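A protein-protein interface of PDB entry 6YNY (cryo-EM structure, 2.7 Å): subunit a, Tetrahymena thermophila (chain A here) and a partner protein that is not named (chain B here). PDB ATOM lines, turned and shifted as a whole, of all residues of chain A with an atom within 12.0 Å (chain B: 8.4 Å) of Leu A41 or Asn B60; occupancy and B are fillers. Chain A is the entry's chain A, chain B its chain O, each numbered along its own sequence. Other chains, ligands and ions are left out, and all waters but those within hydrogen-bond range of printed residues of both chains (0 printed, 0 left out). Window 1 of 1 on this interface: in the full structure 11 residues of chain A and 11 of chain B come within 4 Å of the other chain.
Hydrophobic or aromatic side chains of chain B that line the printed part of chain A: Ile B61, Val B62 and His B63. Along chain B the printed residues that touch a printed residue of chain A span positions 57 to 65. Hydrophobic or aromatic side chains of chain A that line the printed part of chain B: Phe A37, Ile A40, Leu A41 and Val A45.
The backbone NH (N) of Glu A46 is in hydrogen-bond range of the side-chain hydroxyl (OH) of Tyr A49 (2.7 Å). The backbone carbonyl oxygen (O) of Gln B56 sits at hydrogen-bond distance from the side-chain hydroxyl (OG1) of Thr B59 (3.0 Å).
Of the printed residues of chain B, Phe A37 touches His B63 (3.6 Å), Val B64 (3.6 Å) and Pro B65 (3.7 Å). Of chain B, only Thr B58 (3.4 Å), Thr B59 (3.7 Å), Asn B60 (2.9 Å) and Val B62 (3.6 Å) come within 4 Å of Leu A41. Gly A43 touches just one residue of chain B: Thr B58 (2.9 Å). Of the printed residues of chain B, Glu A46 touches Asn B57 and Thr B58. Gln B56 touches none of the printed residues of chain A. Thr B58 touches just these residues of chain A: Leu A41, Gly A43, Gly A44 and Glu A46. Thr B59 touches just one residue of chain A: Leu A41. Printed residues of chain A within 4 Å of Val B62: Ser A38 (3.5 Å), Asp A39 (2.8 Å) and Leu A41 (3.6 Å). Printed residues of chain A within 4 Å of Val B64: Phe A37. The nearest residue of chain B that does not touch Leu A41 is Met B68 (4.3 Å). The nearest residue of chain A that does not touch Asn B60 is Gly A43 (5.2 Å).
N of Val B62 lies within hydrogen-bond range of O of Asp A39, 2.8 Å away. The backbone NH (N) of Leu A41 is in hydrogen-bond range of the backbone carbonyl oxygen (O) of Asn B60, at 2.9 Å. The backbone NH of Gly A43 lies within hydrogen-bond range of the backbone carbonyl oxygen of Thr B58 (2.9 Å). N of Gly A44 is in hydrogen-bond range of O of Thr B58, at 2.7 Å. N of Val A45 lies within hydrogen-bond range of OD1 of Asn B60. The side-chain amide nitrogen of Asn B57 sits close to the side-chain carboxylate of Glu A46 (3.3 Å). OE2 of Glu A46 sits close to N of Thr B58. O of Leu A41 lies close to O of Thr B58, at 3.4 Å.
CD2 of Phe A37 touches O of His B63 (3.6 Å). Pro B65 touches Phe A37 (N to CE2, 3.7 Å). OG of Ser A38 touches CG2 of Ile B61 (3.4 Å). Ser A38 touches Val B62. OG of Ser A38 touches ND1 of His B63 (3.7 Å). O of Asn B60 touches O of Asp A39, 3.8 Å away. Asp A39 touches Ile B61 (O to CA, 3.5 Å). O of Leu A41 touches CA of Thr B59, at 3.7 Å. Leu A41 touches Val B62. Gly A44 touches Asn B60.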
ATOM      1  N   PHE A  37     -27.239   7.740 -21.011  1.00  0.00           N
ATOM      2  CA  PHE A  37     -26.331   8.683 -20.378  1.00  0.00           C
ATOM      3  C   PHE A  37     -25.614   8.026 -19.210  1.00  0.00           C
ATOM      4  O   PHE A  37     -26.202   7.257 -18.446  1.00  0.00           O
ATOM      5  CB  PHE A  37     -27.084   9.918 -19.890  1.00  0.00           C
ATOM      6  CG  PHE A  37     -26.198  10.947 -19.256  1.00  0.00           C
ATOM      7  CD1 PHE A  37     -25.659  11.970 -20.007  1.00  0.00           C
ATOM      8  CD2 PHE A  37     -25.895  10.884 -17.910  1.00  0.00           C
ATOM      9  CE1 PHE A  37     -24.843  12.909 -19.429  1.00  0.00           C
ATOM     10  CE2 PHE A  37     -25.080  11.820 -17.330  1.00  0.00           C
ATOM     11  CZ  PHE A  37     -24.553  12.834 -18.088  1.00  0.00           C
ATOM     12  N   SER A  38     -24.329   8.334 -19.080  1.00  0.00           N
ATOM     13  CA  SER A  38     -23.532   7.845 -17.962  1.00  0.00           C
ATOM     14  C   SER A  38     -22.269   8.683 -17.893  1.00  0.00           C
ATOM     15  O   SER A  38     -21.497   8.714 -18.856  1.00  0.00           O
ATOM     16  CB  SER A  38     -23.202   6.368 -18.132  1.00  0.00           C
ATOM     17  OG  SER A  38     -22.515   5.864 -17.005  1.00  0.00           O
ATOM     18  N   ASP A  39     -22.062   9.361 -16.771  1.00  0.00           N
ATOM     19  CA  ASP A  39     -20.916  10.234 -16.579  1.00  0.00           C
ATOM     20  C   ASP A  39     -20.027   9.675 -15.482  1.00  0.00           C
ATOM     21  O   ASP A  39     -20.516   9.175 -14.464  1.00  0.00           O
ATOM     22  CB  ASP A  39     -21.357  11.651 -16.217  1.00  0.00           C
ATOM     23  CG  ASP A  39     -20.217  12.649 -16.265  1.00  0.00           C
ATOM     24  OD1 ASP A  39     -19.044  12.228 -16.192  1.00  0.00           O
ATOM     25  OD2 ASP A  39     -20.496  13.862 -16.369  1.00  0.00           O
ATOM     26  N   ILE A  40     -18.721   9.761 -15.698  1.00  0.00           N
ATOM     27  CA  ILE A  40     -17.721   9.355 -14.723  1.00  0.00           C
ATOM     28  C   ILE A  40     -17.118  10.611 -14.115  1.00  0.00           C
ATOM     29  O   ILE A  40     -16.742  11.539 -14.840  1.00  0.00           O
ATOM     30  CB  ILE A  40     -16.636   8.469 -15.356  1.00  0.00           C
ATOM     31  CG1 ILE A  40     -15.624   8.042 -14.296  1.00  0.00           C
ATOM     32  CG2 ILE A  40     -15.943   9.190 -16.499  1.00  0.00           C
ATOM     33  CD1 ILE A  40     -14.639   7.025 -14.777  1.00  0.00           C
ATOM     34  N   LEU A  41     -17.044  10.647 -12.793  1.00  0.00           N
ATOM     35  CA  LEU A  41     -16.529  11.796 -12.058  1.00  0.00           C
ATOM     36  C   LEU A  41     -15.221  11.385 -11.396  1.00  0.00           C
ATOM     37  O   LEU A  41     -15.222  10.801 -10.309  1.00  0.00           O
ATOM     38  CB  LEU A  41     -17.541  12.281 -11.028  1.00  0.00           C
ATOM     39  CG  LEU A  41     -18.949  12.553 -11.551  1.00  0.00           C
ATOM     40  CD1 LEU A  41     -19.821  13.092 -10.440  1.00  0.00           C
ATOM     41  CD2 LEU A  41     -18.921  13.510 -12.722  1.00  0.00           C
ATOM     42  N   LEU A  42     -14.107  11.683 -12.056  1.00  0.00           N
ATOM     43  CA  LEU A  42     -12.795  11.496 -11.449  1.00  0.00           C
ATOM     44  C   LEU A  42     -12.640  12.547 -10.365  1.00  0.00           C
ATOM     45  O   LEU A  42     -12.411  13.725 -10.642  1.00  0.00           O
ATOM     46  CB  LEU A  42     -11.687  11.602 -12.490  1.00  0.00           C
ATOM     47  CG  LEU A  42     -11.762  10.639 -13.669  1.00  0.00           C
ATOM     48  CD1 LEU A  42     -10.520  10.786 -14.507  1.00  0.00           C
ATOM     49  CD2 LEU A  42     -11.931   9.212 -13.201  1.00  0.00           C
ATOM     50  N   GLY A  43     -12.776  12.116  -9.121  1.00  0.00           N
ATOM     51  CA  GLY A  43     -12.899  13.022  -8.003  1.00  0.00           C
ATOM     52  C   GLY A  43     -14.343  13.100  -7.563  1.00  0.00           C
ATOM     53  O   GLY A  43     -15.148  13.839  -8.135  1.00  0.00           O
ATOM     54  N   GLY A  44     -14.669  12.336  -6.532  1.00  0.00           N
ATOM     55  CA  GLY A  44     -16.024  12.222  -6.051  1.00  0.00           C
ATOM     56  C   GLY A  44     -16.052  12.015  -4.555  1.00  0.00           C
ATOM     57  O   GLY A  44     -15.341  12.703  -3.817  1.00  0.00           O
ATOM     58  N   VAL A  45     -16.852  11.061  -4.095  1.00  0.00           N
ATOM     59  CA  VAL A  45     -17.067  10.850  -2.673  1.00  0.00           C
ATOM     60  C   VAL A  45     -16.600   9.455  -2.291  1.00  0.00           C
ATOM     61  O   VAL A  45     -16.604   8.526  -3.105  1.00  0.00           O
ATOM     62  CB  VAL A  45     -18.544  11.057  -2.283  1.00  0.00           C
ATOM     63  CG1 VAL A  45     -18.956  12.468  -2.583  1.00  0.00           C
ATOM     64  CG2 VAL A  45     -19.428  10.084  -3.017  1.00  0.00           C
ATOM     65  N   GLU A  46     -16.200   9.318  -1.037  1.00  0.00           N
ATOM     66  CA  GLU A  46     -15.730   8.065  -0.485  1.00  0.00           C
ATOM     67  C   GLU A  46     -16.822   7.432   0.372  1.00  0.00           C
ATOM     68  O   GLU A  46     -17.955   7.918   0.440  1.00  0.00           O
ATOM     69  CB  GLU A  46     -14.450   8.308   0.311  1.00  0.00           C
ATOM     70  CG  GLU A  46     -13.234   8.531  -0.553  1.00  0.00           C
ATOM     71  CD  GLU A  46     -12.786   7.274  -1.262  1.00  0.00           C
ATOM     72  OE1 GLU A  46     -13.176   6.170  -0.827  1.00  0.00           O
ATOM     73  OE2 GLU A  46     -12.047   7.389  -2.260  1.00  0.00           O
ATOM     74  N   TRP A  47     -16.478   6.333   1.042  1.00  0.00           N
ATOM     75  CA  TRP A  47     -17.445   5.627   1.872  1.00  0.00           C
ATOM     76  C   TRP A  47     -17.599   6.291   3.235  1.00  0.00           C
ATOM     77  O   TRP A  47     -18.718   6.594   3.663  1.00  0.00           O
ATOM     78  CB  TRP A  47     -17.024   4.166   2.020  1.00  0.00           C
ATOM     79  CG  TRP A  47     -17.829   3.411   3.006  1.00  0.00           C
ATOM     80  CD1 TRP A  47     -19.172   3.224   2.991  1.00  0.00           C
ATOM     81  CD2 TRP A  47     -17.340   2.725   4.158  1.00  0.00           C
ATOM     82  NE1 TRP A  47     -19.557   2.470   4.066  1.00  0.00           N
ATOM     83  CE2 TRP A  47     -18.448   2.150   4.801  1.00  0.00           C
ATOM     84  CE3 TRP A  47     -16.074   2.545   4.713  1.00  0.00           C
ATOM     85  CZ2 TRP A  47     -18.326   1.409   5.965  1.00  0.00           C
ATOM     86  CZ3 TRP A  47     -15.958   1.812   5.867  1.00  0.00           C
ATOM     87  CH2 TRP A  47     -17.075   1.251   6.482  1.00  0.00           C
ATOM     88  N   VAL A  48     -16.491   6.533   3.927  1.00  0.00           N
ATOM     89  CA  VAL A  48     -16.507   7.154   5.244  1.00  0.00           C
ATOM     90  C   VAL A  48     -15.691   8.433   5.203  1.00  0.00           C
ATOM     91  O   VAL A  48     -14.759   8.580   4.408  1.00  0.00           O
ATOM     92  CB  VAL A  48     -15.968   6.221   6.346  1.00  0.00           C
ATOM     93  CG1 VAL A  48     -17.008   5.212   6.733  1.00  0.00           C
ATOM     94  CG2 VAL A  48     -14.709   5.537   5.883  1.00  0.00           C
ATOM     95  N   TYR A  49     -16.053   9.362   6.079  1.00  0.00           N
ATOM     96  CA  TYR A  49     -15.305  10.591   6.262  1.00  0.00           C
ATOM     97  C   TYR A  49     -15.154  10.858   7.751  1.00  0.00           C
ATOM     98  O   TYR A  49     -15.947  10.395   8.573  1.00  0.00           O
ATOM     99  CB  TYR A  49     -15.982  11.778   5.577  1.00  0.00           C
ATOM    100  CG  TYR A  49     -15.859  11.777   4.076  1.00  0.00           C
ATOM    101  CD1 TYR A  49     -16.952  11.510   3.271  1.00  0.00           C
ATOM    102  CD2 TYR A  49     -14.649  12.046   3.462  1.00  0.00           C
ATOM    103  CE1 TYR A  49     -16.844  11.513   1.902  1.00  0.00           C
ATOM    104  CE2 TYR A  49     -14.532  12.050   2.095  1.00  0.00           C
ATOM    105  CZ  TYR A  49     -15.631  11.783   1.320  1.00  0.00           C
ATOM    106  OH  TYR A  49     -15.517  11.785  -0.047  1.00  0.00           O
ATOM    107  N   MET B  55      -6.891   2.152  -9.683  1.00  0.00           N
ATOM    108  CA  MET B  55      -8.190   2.771  -9.907  1.00  0.00           C
ATOM    109  C   MET B  55      -8.447   3.861  -8.871  1.00  0.00           C
ATOM    110  O   MET B  55      -8.392   3.603  -7.670  1.00  0.00           O
ATOM    111  CB  MET B  55      -9.286   1.720  -9.848  1.00  0.00           C
ATOM    112  CG  MET B  55     -10.611   2.177 -10.422  1.00  0.00           C
ATOM    113  SD  MET B  55     -10.584   2.253 -12.213  1.00  0.00           S
ATOM    114  CE  MET B  55     -12.282   2.689 -12.540  1.00  0.00           C
ATOM    115  N   GLN B  56      -8.729   5.077  -9.337  1.00  0.00           N
ATOM    116  CA  GLN B  56      -8.943   6.195  -8.429  1.00  0.00           C
ATOM    117  C   GLN B  56     -10.007   5.859  -7.396  1.00  0.00           C
ATOM    118  O   GLN B  56     -11.084   5.359  -7.728  1.00  0.00           O
ATOM    119  CB  GLN B  56      -9.352   7.445  -9.203  1.00  0.00           C
ATOM    120  CG  GLN B  56      -8.242   8.106  -9.977  1.00  0.00           C
ATOM    121  CD  GLN B  56      -8.140   7.613 -11.398  1.00  0.00           C
ATOM    122  OE1 GLN B  56      -8.480   6.472 -11.703  1.00  0.00           O
ATOM    123  NE2 GLN B  56      -7.686   8.482 -12.285  1.00  0.00           N
ATOM    124  N   ASN B  57      -9.693   6.148  -6.134  1.00  0.00           N
ATOM    125  CA  ASN B  57     -10.582   5.780  -5.040  1.00  0.00           C
ATOM    126  C   ASN B  57     -11.836   6.642  -5.028  1.00  0.00           C
ATOM    127  O   ASN B  57     -12.925   6.157  -4.700  1.00  0.00           O
ATOM    128  CB  ASN B  57      -9.833   5.886  -3.715  1.00  0.00           C
ATOM    129  CG  ASN B  57      -9.185   7.239  -3.519  1.00  0.00           C
ATOM    130  OD1 ASN B  57      -9.025   8.007  -4.466  1.00  0.00           O
ATOM    131  ND2 ASN B  57      -8.798   7.533  -2.289  1.00  0.00           N
ATOM    132  N   THR B  58     -11.705   7.919  -5.368  1.00  0.00           N
ATOM    133  CA  THR B  58     -12.836   8.843  -5.387  1.00  0.00           C
ATOM    134  C   THR B  58     -13.485   8.902  -6.766  1.00  0.00           C
ATOM    135  O   THR B  58     -13.705   9.973  -7.327  1.00  0.00           O
ATOM    136  CB  THR B  58     -12.379  10.227  -4.944  1.00  0.00           C
ATOM    137  OG1 THR B  58     -11.487  10.776  -5.920  1.00  0.00           O
ATOM    138  CG2 THR B  58     -11.679  10.171  -3.604  1.00  0.00           C
ATOM    139  N   THR B  59     -13.810   7.738  -7.316  1.00  0.00           N
ATOM    140  CA  THR B  59     -14.417   7.622  -8.634  1.00  0.00           C
ATOM    141  C   THR B  59     -15.871   7.202  -8.485  1.00  0.00           C
ATOM    142  O   THR B  59     -16.180   6.279  -7.726  1.00  0.00           O
ATOM    143  CB  THR B  59     -13.663   6.614  -9.499  1.00  0.00           C
ATOM    144  OG1 THR B  59     -12.352   7.112  -9.779  1.00  0.00           O
ATOM    145  CG2 THR B  59     -14.389   6.370 -10.800  1.00  0.00           C
ATOM    146  N   ASN B  60     -16.753   7.880  -9.213  1.00  0.00           N
ATOM    147  CA  ASN B  60     -18.181   7.625  -9.146  1.00  0.00           C
ATOM    148  C   ASN B  60     -18.770   7.643 -10.546  1.00  0.00           C
ATOM    149  O   ASN B  60     -18.386   8.467 -11.379  1.00  0.00           O
ATOM    150  CB  ASN B  60     -18.892   8.667  -8.278  1.00  0.00           C
ATOM    151  CG  ASN B  60     -18.349   8.725  -6.869  1.00  0.00           C
ATOM    152  OD1 ASN B  60     -18.132   9.802  -6.322  1.00  0.00           O
ATOM    153  ND2 ASN B  60     -18.118   7.565  -6.275  1.00  0.00           N
ATOM    154  N   ILE B  61     -19.703   6.731 -10.796  1.00  0.00           N
ATOM    155  CA  ILE B  61     -20.431   6.660 -12.055  1.00  0.00           C
ATOM    156  C   ILE B  61     -21.842   7.160 -11.791  1.00  0.00           C
ATOM    157  O   ILE B  61     -22.589   6.549 -11.019  1.00  0.00           O
ATOM    158  CB  ILE B  61     -20.460   5.237 -12.628  1.00  0.00           C
ATOM    159  CG1 ILE B  61     -19.050   4.654 -12.725  1.00  0.00           C
ATOM    160  CG2 ILE B  61     -21.106   5.247 -13.991  1.00  0.00           C
ATOM    161  CD1 ILE B  61     -18.189   5.293 -13.753  1.00  0.00           C
ATOM    162  N   VAL B  62     -22.208   8.263 -12.433  1.00  0.00           N
ATOM    163  CA  VAL B  62     -23.510   8.888 -12.252  1.00  0.00           C
ATOM    164  C   VAL B  62     -24.328   8.683 -13.515  1.00  0.00           C
ATOM    165  O   VAL B  62     -23.799   8.760 -14.629  1.00  0.00           O
ATOM    166  CB  VAL B  62     -23.372  10.385 -11.917  1.00  0.00           C
ATOM    167  CG1 VAL B  62     -24.709  10.963 -11.541  1.00  0.00           C
ATOM    168  CG2 VAL B  62     -22.385  10.581 -10.792  1.00  0.00           C
ATOM    169  N   HIS B  63     -25.620   8.416 -13.338  1.00  0.00           N
ATOM    170  CA  HIS B  63     -26.522   8.142 -14.446  1.00  0.00           C
ATOM    171  C   HIS B  63     -27.424   9.318 -14.787  1.00  0.00           C
ATOM    172  O   HIS B  63     -28.187   9.231 -15.753  1.00  0.00           O
ATOM    173  CB  HIS B  63     -27.375   6.915 -14.133  1.00  0.00           C
ATOM    174  CG  HIS B  63     -26.603   5.636 -14.100  1.00  0.00           C
ATOM    175  ND1 HIS B  63     -25.406   5.475 -14.761  1.00  0.00           N
ATOM    176  CD2 HIS B  63     -26.854   4.459 -13.483  1.00  0.00           C
ATOM    177  CE1 HIS B  63     -24.953   4.252 -14.554  1.00  0.00           C
ATOM    178  NE2 HIS B  63     -25.814   3.615 -13.782  1.00  0.00           N
ATOM    179  N   VAL B  64     -27.370  10.402 -14.022  1.00  0.00           N
ATOM    180  CA  VAL B  64     -28.138  11.603 -14.335  1.00  0.00           C
ATOM    181  C   VAL B  64     -27.168  12.758 -14.545  1.00  0.00           C
ATOM    182  O   VAL B  64     -26.085  12.771 -13.944  1.00  0.00           O
ATOM    183  CB  VAL B  64     -29.162  11.935 -13.238  1.00  0.00           C
ATOM    184  CG1 VAL B  64     -30.184  10.840 -13.130  1.00  0.00           C
ATOM    185  CG2 VAL B  64     -28.482  12.170 -11.910  1.00  0.00           C
ATOM    186  N   PRO B  65     -27.504  13.738 -15.380  1.00  0.00           N
ATOM    187  CA  PRO B  65     -26.575  14.845 -15.619  1.00  0.00           C
ATOM    188  C   PRO B  65     -26.367  15.695 -14.378  1.00  0.00           C
ATOM    189  O   PRO B  65     -27.300  15.963 -13.619  1.00  0.00           O
ATOM    190  CB  PRO B  65     -27.256  15.645 -16.733  1.00  0.00           C
ATOM    191  CG  PRO B  65     -28.222  14.724 -17.337  1.00  0.00           C
ATOM    192  CD  PRO B  65     -28.686  13.834 -16.247  1.00  0.00           C
ATOM    193  N   VAL B  66     -25.125  16.121 -14.184  1.00  0.00           N
ATOM    194  CA  VAL B  66     -24.758  17.052 -13.129  1.00  0.00           C
ATOM    195  C   VAL B  66     -23.905  18.146 -13.745  1.00  0.00           C
ATOM    196  O   VAL B  66     -23.206  17.928 -14.740  1.00  0.00           O
ATOM    197  CB  VAL B  66     -23.995  16.363 -11.979  1.00  0.00           C
ATOM    198  CG1 VAL B  66     -24.833  15.272 -11.359  1.00  0.00           C
ATOM    199  CG2 VAL B  66     -22.686  15.804 -12.478  1.00  0.00           C
ATOM    200  N   HIS B  67     -23.971  19.333 -13.155  1.00  0.00           N
ATOM    201  CA  HIS B  67     -23.161  20.465 -13.579  1.00  0.00           C
ATOM    202  C   HIS B  67     -22.257  20.874 -12.428  1.00  0.00           C
ATOM    203  O   HIS B  67     -22.739  21.181 -11.334  1.00  0.00           O
ATOM    204  CB  HIS B  67     -24.031  21.639 -14.023  1.00  0.00           C
ATOM    205  CG  HIS B  67     -23.256  22.748 -14.659  1.00  0.00           C
ATOM    206  ND1 HIS B  67     -22.702  23.778 -13.934  1.00  0.00           N
ATOM    207  CD2 HIS B  67     -22.932  22.980 -15.952  1.00  0.00           C
ATOM    208  CE1 HIS B  67     -22.075  24.603 -14.753  1.00  0.00           C
ATOM    209  NE2 HIS B  67     -22.198  24.140 -15.984  1.00  0.00           N
ATOM    210  N   MET B  68     -20.954  20.875 -12.677  1.00  0.00           N
ATOM    211  CA  MET B  68     -19.959  21.191 -11.666  1.00  0.00           C
ATOM    212  C   MET B  68     -19.541  22.650 -11.761  1.00  0.00           C
ATOM    213  O   MET B  68     -19.296  23.170 -12.853  1.00  0.00           O
ATOM    214  CB  MET B  68     -18.738  20.287 -11.818  1.00  0.00           C
ATOM    215  CG  MET B  68     -18.934  18.897 -11.263  1.00  0.00           C
ATOM    216  SD  MET B  68     -18.749  18.850  -9.476  1.00  0.00           S
ATOM    217  CE  MET B  68     -19.022  17.114  -9.162  1.00  0.00           C
ATOM    218  N   ASP B  75     -14.941  22.514  -5.251  1.00  0.00           N
ATOM    219  CA  ASP B  75     -15.477  21.579  -6.231  1.00  0.00           C
ATOM    220  C   ASP B  75     -16.805  21.059  -5.709  1.00  0.00           C
ATOM    221  O   ASP B  75     -16.858  20.472  -4.625  1.00  0.00           O
ATOM    222  CB  ASP B  75     -14.516  20.415  -6.483  1.00  0.00           C
ATOM    223  CG  ASP B  75     -15.008  19.480  -7.566  1.00  0.00           C
ATOM    224  OD1 ASP B  75     -15.962  19.848  -8.280  1.00  0.00           O
ATOM    225  OD2 ASP B  75     -14.448  18.372  -7.699  1.00  0.00           O
ATOM    226  N   ILE B  77     -21.350  20.388  -6.990  1.00  0.00           N
ATOM    227  CA  ILE B  77     -22.418  20.372  -7.982  1.00  0.00           C
ATOM    228  C   ILE B  77     -23.288  21.599  -7.745  1.00  0.00           C
ATOM    229  O   ILE B  77     -24.024  21.668  -6.760  1.00  0.00           O
ATOM    230  CB  ILE B  77     -23.236  19.080  -7.898  1.00  0.00           C
ATOM    231  CG1 ILE B  77     -22.370  17.885  -8.288  1.00  0.00           C
ATOM    232  CG2 ILE B  77     -24.450  19.165  -8.784  1.00  0.00           C
ATOM    233  CD1 ILE B  77     -22.928  16.569  -7.853  1.00  0.00           C
